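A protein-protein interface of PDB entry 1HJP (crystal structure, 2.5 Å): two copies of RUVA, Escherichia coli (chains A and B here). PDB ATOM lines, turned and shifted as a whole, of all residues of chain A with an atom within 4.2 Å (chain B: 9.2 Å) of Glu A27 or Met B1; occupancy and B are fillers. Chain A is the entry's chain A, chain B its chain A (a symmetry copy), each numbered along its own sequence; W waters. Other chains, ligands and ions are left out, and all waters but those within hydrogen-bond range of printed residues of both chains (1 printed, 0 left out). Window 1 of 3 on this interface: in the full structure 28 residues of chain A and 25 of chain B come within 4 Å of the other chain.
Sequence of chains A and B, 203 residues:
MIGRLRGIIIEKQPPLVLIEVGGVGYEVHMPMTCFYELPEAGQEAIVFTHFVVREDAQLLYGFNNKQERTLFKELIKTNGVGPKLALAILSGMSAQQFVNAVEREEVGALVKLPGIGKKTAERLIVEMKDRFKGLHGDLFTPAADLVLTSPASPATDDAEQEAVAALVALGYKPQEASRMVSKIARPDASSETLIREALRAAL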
ATOM      1  N   VAL A  17     -19.434  21.280  37.584  1.00  0.00           N
ATOM      2  CA  VAL A  17     -20.601  22.141  37.543  1.00  0.00           C
ATOM      3  C   VAL A  17     -20.397  23.039  36.295  1.00  0.00           C
ATOM      4  O   VAL A  17     -19.266  23.443  36.004  1.00  0.00           O
ATOM      5  CB  VAL A  17     -20.818  23.169  38.664  1.00  0.00           C
ATOM      6  CG1 VAL A  17     -22.287  23.271  39.034  1.00  0.00           C
ATOM      7  CG2 VAL A  17     -19.903  22.950  39.835  1.00  0.00           C
ATOM      8  N   LEU A  18     -21.501  23.437  35.694  1.00  0.00           N
ATOM      9  CA  LEU A  18     -21.395  24.350  34.565  1.00  0.00           C
ATOM     10  C   LEU A  18     -22.099  25.627  35.003  1.00  0.00           C
ATOM     11  O   LEU A  18     -23.322  25.638  35.242  1.00  0.00           O
ATOM     12  CB  LEU A  18     -21.960  23.749  33.291  1.00  0.00           C
ATOM     13  CG  LEU A  18     -21.796  24.580  32.010  1.00  0.00           C
ATOM     14  CD1 LEU A  18     -20.341  24.702  31.616  1.00  0.00           C
ATOM     15  CD2 LEU A  18     -22.613  23.941  30.891  1.00  0.00           C
ATOM     16  N   GLY A  25     -20.125  29.743  29.599  1.00  0.00           N
ATOM     17  CA  GLY A  25     -20.363  28.604  30.451  1.00  0.00           C
ATOM     18  C   GLY A  25     -19.053  28.042  30.975  1.00  0.00           C
ATOM     19  O   GLY A  25     -18.378  27.325  30.241  1.00  0.00           O
ATOM     20  N   TYR A  26     -18.742  28.322  32.252  1.00  0.00           N
ATOM     21  CA  TYR A  26     -17.483  27.825  32.800  1.00  0.00           C
ATOM     22  C   TYR A  26     -17.641  26.444  33.406  1.00  0.00           C
ATOM     23  O   TYR A  26     -18.614  26.206  34.113  1.00  0.00           O
ATOM     24  CB  TYR A  26     -16.888  28.758  33.863  1.00  0.00           C
ATOM     25  CG  TYR A  26     -16.359  30.051  33.287  1.00  0.00           C
ATOM     26  CD1 TYR A  26     -15.101  30.142  32.725  1.00  0.00           C
ATOM     27  CD2 TYR A  26     -17.158  31.179  33.262  1.00  0.00           C
ATOM     28  CE1 TYR A  26     -14.647  31.321  32.160  1.00  0.00           C
ATOM     29  CE2 TYR A  26     -16.714  32.363  32.715  1.00  0.00           C
ATOM     30  CZ  TYR A  26     -15.463  32.425  32.169  1.00  0.00           C
ATOM     31  OH  TYR A  26     -15.026  33.618  31.644  1.00  0.00           O
ATOM     32  N   GLU A  27     -16.692  25.567  33.134  1.00  0.00           N
ATOM     33  CA  GLU A  27     -16.664  24.255  33.744  1.00  0.00           C
ATOM     34  C   GLU A  27     -15.871  24.365  35.045  1.00  0.00           C
ATOM     35  O   GLU A  27     -14.670  24.645  34.961  1.00  0.00           O
ATOM     36  CB  GLU A  27     -15.966  23.215  32.870  1.00  0.00           C
ATOM     37  CG  GLU A  27     -16.781  22.956  31.621  1.00  0.00           C
ATOM     38  CD  GLU A  27     -16.182  21.935  30.688  1.00  0.00           C
ATOM     39  OE1 GLU A  27     -14.975  21.655  30.766  1.00  0.00           O
ATOM     40  OE2 GLU A  27     -16.977  21.420  29.872  1.00  0.00           O
ATOM     41  N   VAL A  28     -16.525  24.148  36.170  1.00  0.00           N
ATOM     42  CA  VAL A  28     -15.847  24.226  37.461  1.00  0.00           C
ATOM     43  C   VAL A  28     -15.768  22.838  38.091  1.00  0.00           C
ATOM     44  O   VAL A  28     -16.800  22.148  38.167  1.00  0.00           O
ATOM     45  CB  VAL A  28     -16.623  25.168  38.403  1.00  0.00           C
ATOM     46  CG1 VAL A  28     -15.971  25.253  39.770  1.00  0.00           C
ATOM     47  CG2 VAL A  28     -16.771  26.560  37.781  1.00  0.00           C
ATOM     48  N   HIS A  29     -14.580  22.429  38.513  1.00  0.00           N
ATOM     49  CA  HIS A  29     -14.394  21.140  39.160  1.00  0.00           C
ATOM     50  C   HIS A  29     -14.453  21.349  40.673  1.00  0.00           C
ATOM     51  O   HIS A  29     -13.632  22.127  41.182  1.00  0.00           O
ATOM     52  CB  HIS A  29     -13.051  20.506  38.808  1.00  0.00           C
ATOM     53  CG  HIS A  29     -12.847  20.284  37.344  1.00  0.00           C
ATOM     54  ND1 HIS A  29     -12.760  19.025  36.794  1.00  0.00           N
ATOM     55  CD2 HIS A  29     -12.709  21.171  36.316  1.00  0.00           C
ATOM     56  CE1 HIS A  29     -12.573  19.153  35.490  1.00  0.00           C
ATOM     57  NE2 HIS A  29     -12.540  20.436  35.174  1.00  0.00           N
ATOM     58  N   PHE A  51      -7.558  28.826  39.629  1.00  0.00           N
ATOM     59  CA  PHE A  51      -7.280  28.635  38.214  1.00  0.00           C
ATOM     60  C   PHE A  51      -5.995  27.848  38.055  1.00  0.00           C
ATOM     61  O   PHE A  51      -5.015  28.394  38.554  1.00  0.00           O
ATOM     62  CB  PHE A  51      -7.164  30.010  37.578  1.00  0.00           C
ATOM     63  CG  PHE A  51      -7.023  30.145  36.097  1.00  0.00           C
ATOM     64  CD1 PHE A  51      -7.674  29.295  35.213  1.00  0.00           C
ATOM     65  CD2 PHE A  51      -6.249  31.179  35.575  1.00  0.00           C
ATOM     66  CE1 PHE A  51      -7.553  29.454  33.847  1.00  0.00           C
ATOM     67  CE2 PHE A  51      -6.129  31.340  34.205  1.00  0.00           C
ATOM     68  CZ  PHE A  51      -6.773  30.473  33.336  1.00  0.00           C
ATOM     69  N   GLN A  58      -6.426  24.563  30.649  1.00  0.00           N
ATOM     70  CA  GLN A  58      -6.728  25.629  31.589  1.00  0.00           C
ATOM     71  C   GLN A  58      -7.984  25.248  32.373  1.00  0.00           C
ATOM     72  O   GLN A  58      -9.054  25.071  31.778  1.00  0.00           O
ATOM     73  CB  GLN A  58      -6.958  26.944  30.866  1.00  0.00           C
ATOM     74  CG  GLN A  58      -5.673  27.594  30.380  1.00  0.00           C
ATOM     75  CD  GLN A  58      -5.923  28.967  29.779  1.00  0.00           C
ATOM     76  OE1 GLN A  58      -4.959  29.484  29.204  1.00  0.00           O
ATOM     77  NE2 GLN A  58      -7.132  29.527  29.905  1.00  0.00           N
ATOM     78  N   LEU A  60     -10.495  25.383  36.122  1.00  0.00           N
ATOM     79  CA  LEU A  60     -11.042  26.035  37.285  1.00  0.00           C
ATOM     80  C   LEU A  60     -11.475  25.001  38.335  1.00  0.00           C
ATOM     81  O   LEU A  60     -12.291  24.116  38.072  1.00  0.00           O
ATOM     82  CB  LEU A  60     -12.223  26.869  36.876  1.00  0.00           C
ATOM     83  CG  LEU A  60     -12.285  28.376  36.753  1.00  0.00           C
ATOM     84  CD1 LEU A  60     -10.965  29.100  36.840  1.00  0.00           C
ATOM     85  CD2 LEU A  60     -12.980  28.693  35.424  1.00  0.00           C
ATOM     86  N   MET B   1     -11.436  25.346  30.160  1.00  0.00           N
ATOM     87  CA  MET B   1     -12.473  25.746  31.145  1.00  0.00           C
ATOM     88  C   MET B   1     -13.771  26.235  30.523  1.00  0.00           C
ATOM     89  O   MET B   1     -14.756  26.417  31.248  1.00  0.00           O
ATOM     90  CB  MET B   1     -11.886  26.825  32.053  1.00  0.00           C
ATOM     91  CG  MET B   1     -11.695  28.165  31.374  1.00  0.00           C
ATOM     92  SD  MET B   1     -10.908  29.377  32.468  1.00  0.00           S
ATOM     93  CE  MET B   1     -10.710  30.740  31.325  1.00  0.00           C
ATOM     94  N   ILE B   2     -13.760  26.523  29.222  1.00  0.00           N
ATOM     95  CA  ILE B   2     -14.957  27.045  28.561  1.00  0.00           C
ATOM     96  C   ILE B   2     -15.739  25.863  27.990  1.00  0.00           C
ATOM     97  O   ILE B   2     -15.295  25.216  27.040  1.00  0.00           O
ATOM     98  CB  ILE B   2     -14.668  28.077  27.461  1.00  0.00           C
ATOM     99  CG1 ILE B   2     -13.807  29.215  27.997  1.00  0.00           C
ATOM    100  CG2 ILE B   2     -15.983  28.609  26.903  1.00  0.00           C
ATOM    101  CD1 ILE B   2     -13.736  30.488  27.173  1.00  0.00           C
ATOM    102  N   GLY B   3     -16.886  25.579  28.595  1.00  0.00           N
ATOM    103  CA  GLY B   3     -17.695  24.455  28.204  1.00  0.00           C
ATOM    104  C   GLY B   3     -18.916  24.776  27.378  1.00  0.00           C
ATOM    105  O   GLY B   3     -19.456  23.883  26.716  1.00  0.00           O
ATOM    106  N   ARG B   4     -19.378  26.011  27.369  1.00  0.00           N
ATOM    107  CA  ARG B   4     -20.572  26.361  26.617  1.00  0.00           C
ATOM    108  C   ARG B   4     -20.582  27.837  26.258  1.00  0.00           C
ATOM    109  O   ARG B   4     -20.203  28.648  27.100  1.00  0.00           O
ATOM    110  CB  ARG B   4     -21.842  26.069  27.438  1.00  0.00           C
ATOM    111  CG  ARG B   4     -23.037  25.778  26.545  1.00  0.00           C
ATOM    112  CD  ARG B   4     -24.305  25.491  27.335  1.00  0.00           C
ATOM    113  NE  ARG B   4     -24.924  26.760  27.665  1.00  0.00           N
ATOM    114  CZ  ARG B   4     -26.173  26.966  28.045  1.00  0.00           C
ATOM    115  NH1 ARG B   4     -27.022  25.966  28.160  1.00  0.00           N
ATOM    116  NH2 ARG B   4     -26.557  28.204  28.317  1.00  0.00           N
ATOM    117  N   LEU B   5     -21.041  28.154  25.054  1.00  0.00           N
ATOM    118  CA  LEU B   5     -21.187  29.551  24.664  1.00  0.00           C
ATOM    119  C   LEU B   5     -22.652  29.713  24.266  1.00  0.00           C
ATOM    120  O   LEU B   5     -23.251  28.833  23.636  1.00  0.00           O
ATOM    121  CB  LEU B   5     -20.287  30.027  23.529  1.00  0.00           C
ATOM    122  CG  LEU B   5     -18.783  30.086  23.832  1.00  0.00           C
ATOM    123  CD1 LEU B   5     -17.974  30.388  22.586  1.00  0.00           C
ATOM    124  CD2 LEU B   5     -18.435  31.104  24.912  1.00  0.00           C
ATOM    125  N   TYR B  26     -16.408  35.145  19.575  1.00  0.00           N
ATOM    126  CA  TYR B  26     -15.596  33.932  19.620  1.00  0.00           C
ATOM    127  C   TYR B  26     -15.615  33.196  18.293  1.00  0.00           C
ATOM    128  O   TYR B  26     -16.677  33.057  17.698  1.00  0.00           O
ATOM    129  CB  TYR B  26     -16.040  32.960  20.721  1.00  0.00           C
ATOM    130  CG  TYR B  26     -15.728  33.460  22.112  1.00  0.00           C
ATOM    131  CD1 TYR B  26     -14.482  33.299  22.686  1.00  0.00           C
ATOM    132  CD2 TYR B  26     -16.685  34.149  22.834  1.00  0.00           C
ATOM    133  CE1 TYR B  26     -14.196  33.802  23.943  1.00  0.00           C
ATOM    134  CE2 TYR B  26     -16.419  34.644  24.092  1.00  0.00           C
ATOM    135  CZ  TYR B  26     -15.178  34.467  24.637  1.00  0.00           C
ATOM    136  OH  TYR B  26     -14.933  34.949  25.901  1.00  0.00           O
ATOM    137  N   VAL B  47     -23.773  26.511  21.894  1.00  0.00           N
ATOM    138  CA  VAL B  47     -22.875  25.478  21.388  1.00  0.00           C
ATOM    139  C   VAL B  47     -22.065  24.945  22.564  1.00  0.00           C
ATOM    140  O   VAL B  47     -21.701  25.679  23.480  1.00  0.00           O
ATOM    141  CB  VAL B  47     -21.956  25.900  20.232  1.00  0.00           C
ATOM    142  CG1 VAL B  47     -22.698  26.591  19.089  1.00  0.00           C
ATOM    143  CG2 VAL B  47     -20.839  26.816  20.692  1.00  0.00           C
ATOM    144  N   PHE B  48     -21.821  23.654  22.543  1.00  0.00           N
ATOM    145  CA  PHE B  48     -21.040  22.963  23.558  1.00  0.00           C
ATOM    146  C   PHE B  48     -19.609  23.031  23.061  1.00  0.00           C
ATOM    147  O   PHE B  48     -19.473  22.799  21.854  1.00  0.00           O
ATOM    148  CB  PHE B  48     -21.505  21.501  23.735  1.00  0.00           C
ATOM    149  CG  PHE B  48     -22.700  21.542  24.657  1.00  0.00           C
ATOM    150  CD1 PHE B  48     -22.509  21.498  26.024  1.00  0.00           C
ATOM    151  CD2 PHE B  48     -23.970  21.690  24.130  1.00  0.00           C
ATOM    152  CE1 PHE B  48     -23.613  21.596  26.867  1.00  0.00           C
ATOM    153  CE2 PHE B  48     -25.062  21.774  24.983  1.00  0.00           C
ATOM    154  CZ  PHE B  48     -24.893  21.731  26.350  1.00  0.00           C
ATOM    155  N   THR B  49     -18.652  23.422  23.902  1.00  0.00           N
ATOM    156  CA  THR B  49     -17.319  23.611  23.345  1.00  0.00           C
ATOM    157  C   THR B  49     -16.244  22.796  24.028  1.00  0.00           C
ATOM    158  O   THR B  49     -16.357  22.316  25.136  1.00  0.00           O
ATOM    159  CB  THR B  49     -16.881  25.099  23.418  1.00  0.00           C
ATOM    160  OG1 THR B  49     -17.027  25.505  24.788  1.00  0.00           O
ATOM    161  CG2 THR B  49     -17.691  26.005  22.519  1.00  0.00           C
ATOM    162  N   HIS B  50     -15.156  22.668  23.293  1.00  0.00           N
ATOM    163  CA  HIS B  50     -13.953  21.986  23.721  1.00  0.00           C
ATOM    164  C   HIS B  50     -12.794  22.954  23.424  1.00  0.00           C
ATOM    165  O   HIS B  50     -12.477  23.342  22.296  1.00  0.00           O
ATOM    166  CB  HIS B  50     -13.772  20.630  23.059  1.00  0.00           C
ATOM    167  CG  HIS B  50     -12.483  19.985  23.476  1.00  0.00           C
ATOM    168  ND1 HIS B  50     -12.286  19.508  24.746  1.00  0.00           N
ATOM    169  CD2 HIS B  50     -11.330  19.755  22.799  1.00  0.00           C
ATOM    170  CE1 HIS B  50     -11.066  19.006  24.839  1.00  0.00           C
ATOM    171  NE2 HIS B  50     -10.467  19.136  23.677  1.00  0.00           N
ATOM    172  N   PHE B  51     -12.193  23.413  24.510  1.00  0.00           N
ATOM    173  CA  PHE B  51     -11.124  24.397  24.431  1.00  0.00           C
ATOM    174  C   PHE B  51      -9.803  23.689  24.213  1.00  0.00           C
ATOM    175  O   PHE B  51      -9.511  22.897  25.105  1.00  0.00           O
ATOM    176  CB  PHE B  51     -11.119  25.177  25.735  1.00  0.00           C
ATOM    177  CG  PHE B  51     -10.222  26.361  25.901  1.00  0.00           C
ATOM    178  CD1 PHE B  51      -9.949  27.232  24.855  1.00  0.00           C
ATOM    179  CD2 PHE B  51      -9.671  26.631  27.151  1.00  0.00           C
ATOM    180  CE1 PHE B  51      -9.140  28.336  25.036  1.00  0.00           C
ATOM    181  CE2 PHE B  51      -8.860  27.739  27.334  1.00  0.00           C
ATOM    182  CZ  PHE B  51      -8.584  28.590  26.275  1.00  0.00           C
ATOM    183  N   VAL B  52      -9.076  23.912  23.125  1.00  0.00           N
ATOM    184  CA  VAL B  52      -7.764  23.274  23.049  1.00  0.00           C
ATOM    185  C   VAL B  52      -6.746  24.403  23.254  1.00  0.00           C
ATOM    186  O   VAL B  52      -6.775  25.452  22.631  1.00  0.00           O
ATOM    187  CB  VAL B  52      -7.414  22.352  21.898  1.00  0.00           C
ATOM    188  CG1 VAL B  52      -8.589  22.111  20.981  1.00  0.00           C
ATOM    189  CG2 VAL B  52      -6.177  22.778  21.120  1.00  0.00           C
ATOM    190  N   VAL B  53      -5.904  24.155  24.245  1.00  0.00           N
ATOM    191  CA  VAL B  53      -4.886  25.111  24.656  1.00  0.00           C
ATOM    192  C   VAL B  53      -3.530  24.642  24.168  1.00  0.00           C
ATOM    193  O   VAL B  53      -3.135  23.493  24.329  1.00  0.00           O
ATOM    194  CB  VAL B  53      -4.891  25.279  26.183  1.00  0.00           C
ATOM    195  CG1 VAL B  53      -3.712  26.110  26.638  1.00  0.00           C
ATOM    196  CG2 VAL B  53      -6.213  25.914  26.604  1.00  0.00           C
ATOM    197  N   GLN B  58      -4.913  29.283  20.954  1.00  0.00           N
ATOM    198  CA  GLN B  58      -6.014  28.905  21.824  1.00  0.00           C
ATOM    199  C   GLN B  58      -7.290  28.815  20.987  1.00  0.00           C
ATOM    200  O   GLN B  58      -7.714  29.816  20.397  1.00  0.00           O
ATOM    201  CB  GLN B  58      -6.205  29.922  22.935  1.00  0.00           C
ATOM    202  CG  GLN B  58      -5.161  29.812  24.034  1.00  0.00           C
ATOM    203  CD  GLN B  58      -5.453  30.751  25.192  1.00  0.00           C
ATOM    204  OE1 GLN B  58      -4.561  30.849  26.042  1.00  0.00           O
ATOM    205  NE2 GLN B  58      -6.625  31.395  25.232  1.00  0.00           N
ATOM    206  N   LEU B  59      -7.866  27.623  20.913  1.00  0.00           N
ATOM    207  CA  LEU B  59      -8.983  27.319  20.059  1.00  0.00           C
ATOM    208  C   LEU B  59     -10.202  26.672  20.695  1.00  0.00           C
ATOM    209  O   LEU B  59     -10.168  25.796  21.552  1.00  0.00           O
ATOM    210  CB  LEU B  59      -8.470  26.321  18.996  1.00  0.00           C
ATOM    211  CG  LEU B  59      -7.468  26.845  17.974  1.00  0.00           C
ATOM    212  CD1 LEU B  59      -6.291  25.893  17.809  1.00  0.00           C
ATOM    213  CD2 LEU B  59      -8.139  27.038  16.629  1.00  0.00           C
ATOM    214  N   LEU B  60     -11.355  27.036  20.157  1.00  0.00           N
ATOM    215  CA  LEU B  60     -12.635  26.505  20.551  1.00  0.00           C
ATOM    216  C   LEU B  60     -13.224  25.622  19.440  1.00  0.00           C
ATOM    217  O   LEU B  60     -13.413  26.057  18.304  1.00  0.00           O
ATOM    218  CB  LEU B  60     -13.572  27.640  20.849  1.00  0.00           C
ATOM    219  CG  LEU B  60     -14.034  28.118  22.209  1.00  0.00           C
ATOM    220  CD1 LEU B  60     -13.309  27.533  23.395  1.00  0.00           C
ATOM    221  CD2 LEU B  60     -13.919  29.646  22.215  1.00  0.00           C
ATOM    222  N   LYS B  66     -23.822  17.424  23.879  1.00  0.00           N
ATOM    223  CA  LYS B  66     -22.721  16.837  24.616  1.00  0.00           C
ATOM    224  C   LYS B  66     -22.222  15.512  24.065  1.00  0.00           C
ATOM    225  O   LYS B  66     -21.048  15.196  24.281  1.00  0.00           O
ATOM    226  CB  LYS B  66     -23.074  16.612  26.089  1.00  0.00           C
ATOM    227  CG  LYS B  66     -22.830  17.765  27.031  1.00  0.00           C
ATOM    228  CD  LYS B  66     -24.152  18.235  27.633  1.00  0.00           C
ATOM    229  CE  LYS B  66     -24.483  17.473  28.905  1.00  0.00           C
ATOM    230  NZ  LYS B  66     -23.261  16.938  29.574  1.00  0.00           N
ATOM    231  N   ARG B  69     -19.616  16.196  21.392  1.00  0.00           N
ATOM    232  CA  ARG B  69     -18.367  16.646  22.006  1.00  0.00           C
ATOM    233  C   ARG B  69     -17.574  15.503  22.618  1.00  0.00           C
ATOM    234  O   ARG B  69     -16.339  15.437  22.542  1.00  0.00           O
ATOM    235  CB  ARG B  69     -18.685  17.674  23.102  1.00  0.00           C
ATOM    236  CG  ARG B  69     -17.519  18.579  23.465  1.00  0.00           C
ATOM    237  CD  ARG B  69     -17.351  18.681  24.967  1.00  0.00           C
ATOM    238  NE  ARG B  69     -18.109  19.735  25.548  1.00  0.00           N
ATOM    239  CZ  ARG B  69     -18.834  19.931  26.613  1.00  0.00           C
ATOM    240  NH1 ARG B  69     -19.097  19.012  27.517  1.00  0.00           N
ATOM    241  NH2 ARG B  69     -19.368  21.142  26.805  1.00  0.00           N
ATOM    242  N   LYS B  73     -13.953  14.344  21.789  1.00  0.00           N
ATOM    243  CA  LYS B  73     -12.927  14.229  22.821  1.00  0.00           C
ATOM    244  C   LYS B  73     -12.336  12.826  22.811  1.00  0.00           C
ATOM    245  O   LYS B  73     -11.125  12.671  22.955  1.00  0.00           O
ATOM    246  CB  LYS B  73     -13.456  14.576  24.202  1.00  0.00           C
ATOM    247  CG  LYS B  73     -13.476  16.057  24.563  1.00  0.00           C
ATOM    248  CD  LYS B  73     -14.666  16.352  25.470  1.00  0.00           C
ATOM    249  CE  LYS B  73     -14.279  17.050  26.758  1.00  0.00           C
ATOM    250  NZ  LYS B  73     -14.248  18.544  26.611  1.00  0.00           N
HETATM  251  O   HOH W   1     -15.303  20.759  27.411  1.00  0.00           O
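Met B1 touches Gly A25.
Ile B2 touches Gly A25 (C to O, 3.8 Å).
Tyr A26 touches Met B1.
OE2 of Glu A27 touches CA of Gly B3 (3.5 Å).
Phe A51 touches Met B1.
Phe B51 touches Gln A58.
Leu A60 touches Met B1.
Of the 19 printed residues of chain B, 7 touch a printed residue of chain A.
Hydrophobic or aromatic side chains of chain B that line the printed part of chain A: Met B1 and Phe B51.
Of the 10 printed residues of chain A, 6 touch a printed residue of chain B.
Printed residues of chain A that touch a printed residue of chain B: Gly A25, Tyr A26, Glu A27, Phe A51, Gln A58 and Leu A60.
Hydrophobic or aromatic side chains of chain A that line the printed part of chain B: Phe A51 and Leu A60.
Among the printed residues, Asp or Glu carboxylates within 4 Å of a Lys or Arg side-chain nitrogen of the other chain: Glu A27 with Arg B69 (3.9 Å).
The backbone NH of Gly B3 sits at hydrogen-bond distance from the backbone carbonyl oxygen of Gly A25 (2.8 Å).
The backbone NH (N) of Gly A25 sits at hydrogen-bond distance from the backbone carbonyl oxygen (O) of Arg B4 (2.7 Å).
The backbone NH (N) of Glu A27 is in hydrogen-bond range of the backbone carbonyl oxygen (O) of Met B1 (2.8 Å).
The side-chain carboxylate of Glu A27 is in salt-bridge range of the guanidinium group of Arg B69, 3.9 Å away.
The backbone carbonyl oxygen (O) of Gln A58 lies within hydrogen-bond range of the backbone NH (N) of Met B1, at 2.9 Å.
The side-chain amide oxygen of Gln B58 sits close to the side-chain amide oxygen of Gln A58 (3.5 Å).
Water W1 lies within hydrogen-bond range of the side-chain amino group of Lys B73 (2.6 Å), the backbone carbonyl oxygen of Thr B49 (3.0 Å) and the side-chain carboxylate of Glu A27 (3.0 Å).
The backbone carbonyl oxygen (O) of Leu A60 sits at hydrogen-bond distance from the backbone NH (N) of His A29.
O of Ile B2 lies within hydrogen-bond range of OG1 of Thr B49 (2.9 Å).
The backbone NH of Thr B49 is in hydrogen-bond range of the backbone carbonyl oxygen of Gly B3, 3.0 Å away.
The backbone carbonyl oxygen (O) of Gly B3 is in hydrogen-bond range of the guanidinium group (NH2) of Arg B69 (2.7 Å).
O of Thr B49 lies within hydrogen-bond range of NE of Arg B69 (3.1 Å).
Glu A27 touches three residues of chain B.
Leu A60 touches just one residue of chain B: Met B1 (3.7 Å).
Of the printed residues of chain A, Arg B69 touches Glu A27.
Of the printed residues of chain A, Phe B51 touches Gln A58 (3.6 Å).
The nearest residue of chain B that does not touch Glu A27 is Ile B2 (4.8 Å).
The nearest printed residue of chain A that does not touch Met B1 is Val A28 (5.7 Å).
The nearest printed residue of chain A that does not touch Phe B51 is Phe A51 (6.9 Å).
Gln A58 touches Phe B51, but with the chains exchanged Phe A51 does not touch Gln B58 (7.6 Å).
Gln A58 touches its own counterpart, Gln B58.
4 positions are printed for both chains.
Of the 13 pairs that touch across the chains among the printed residues, 1 has its exchanged pair printed and touching as well.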
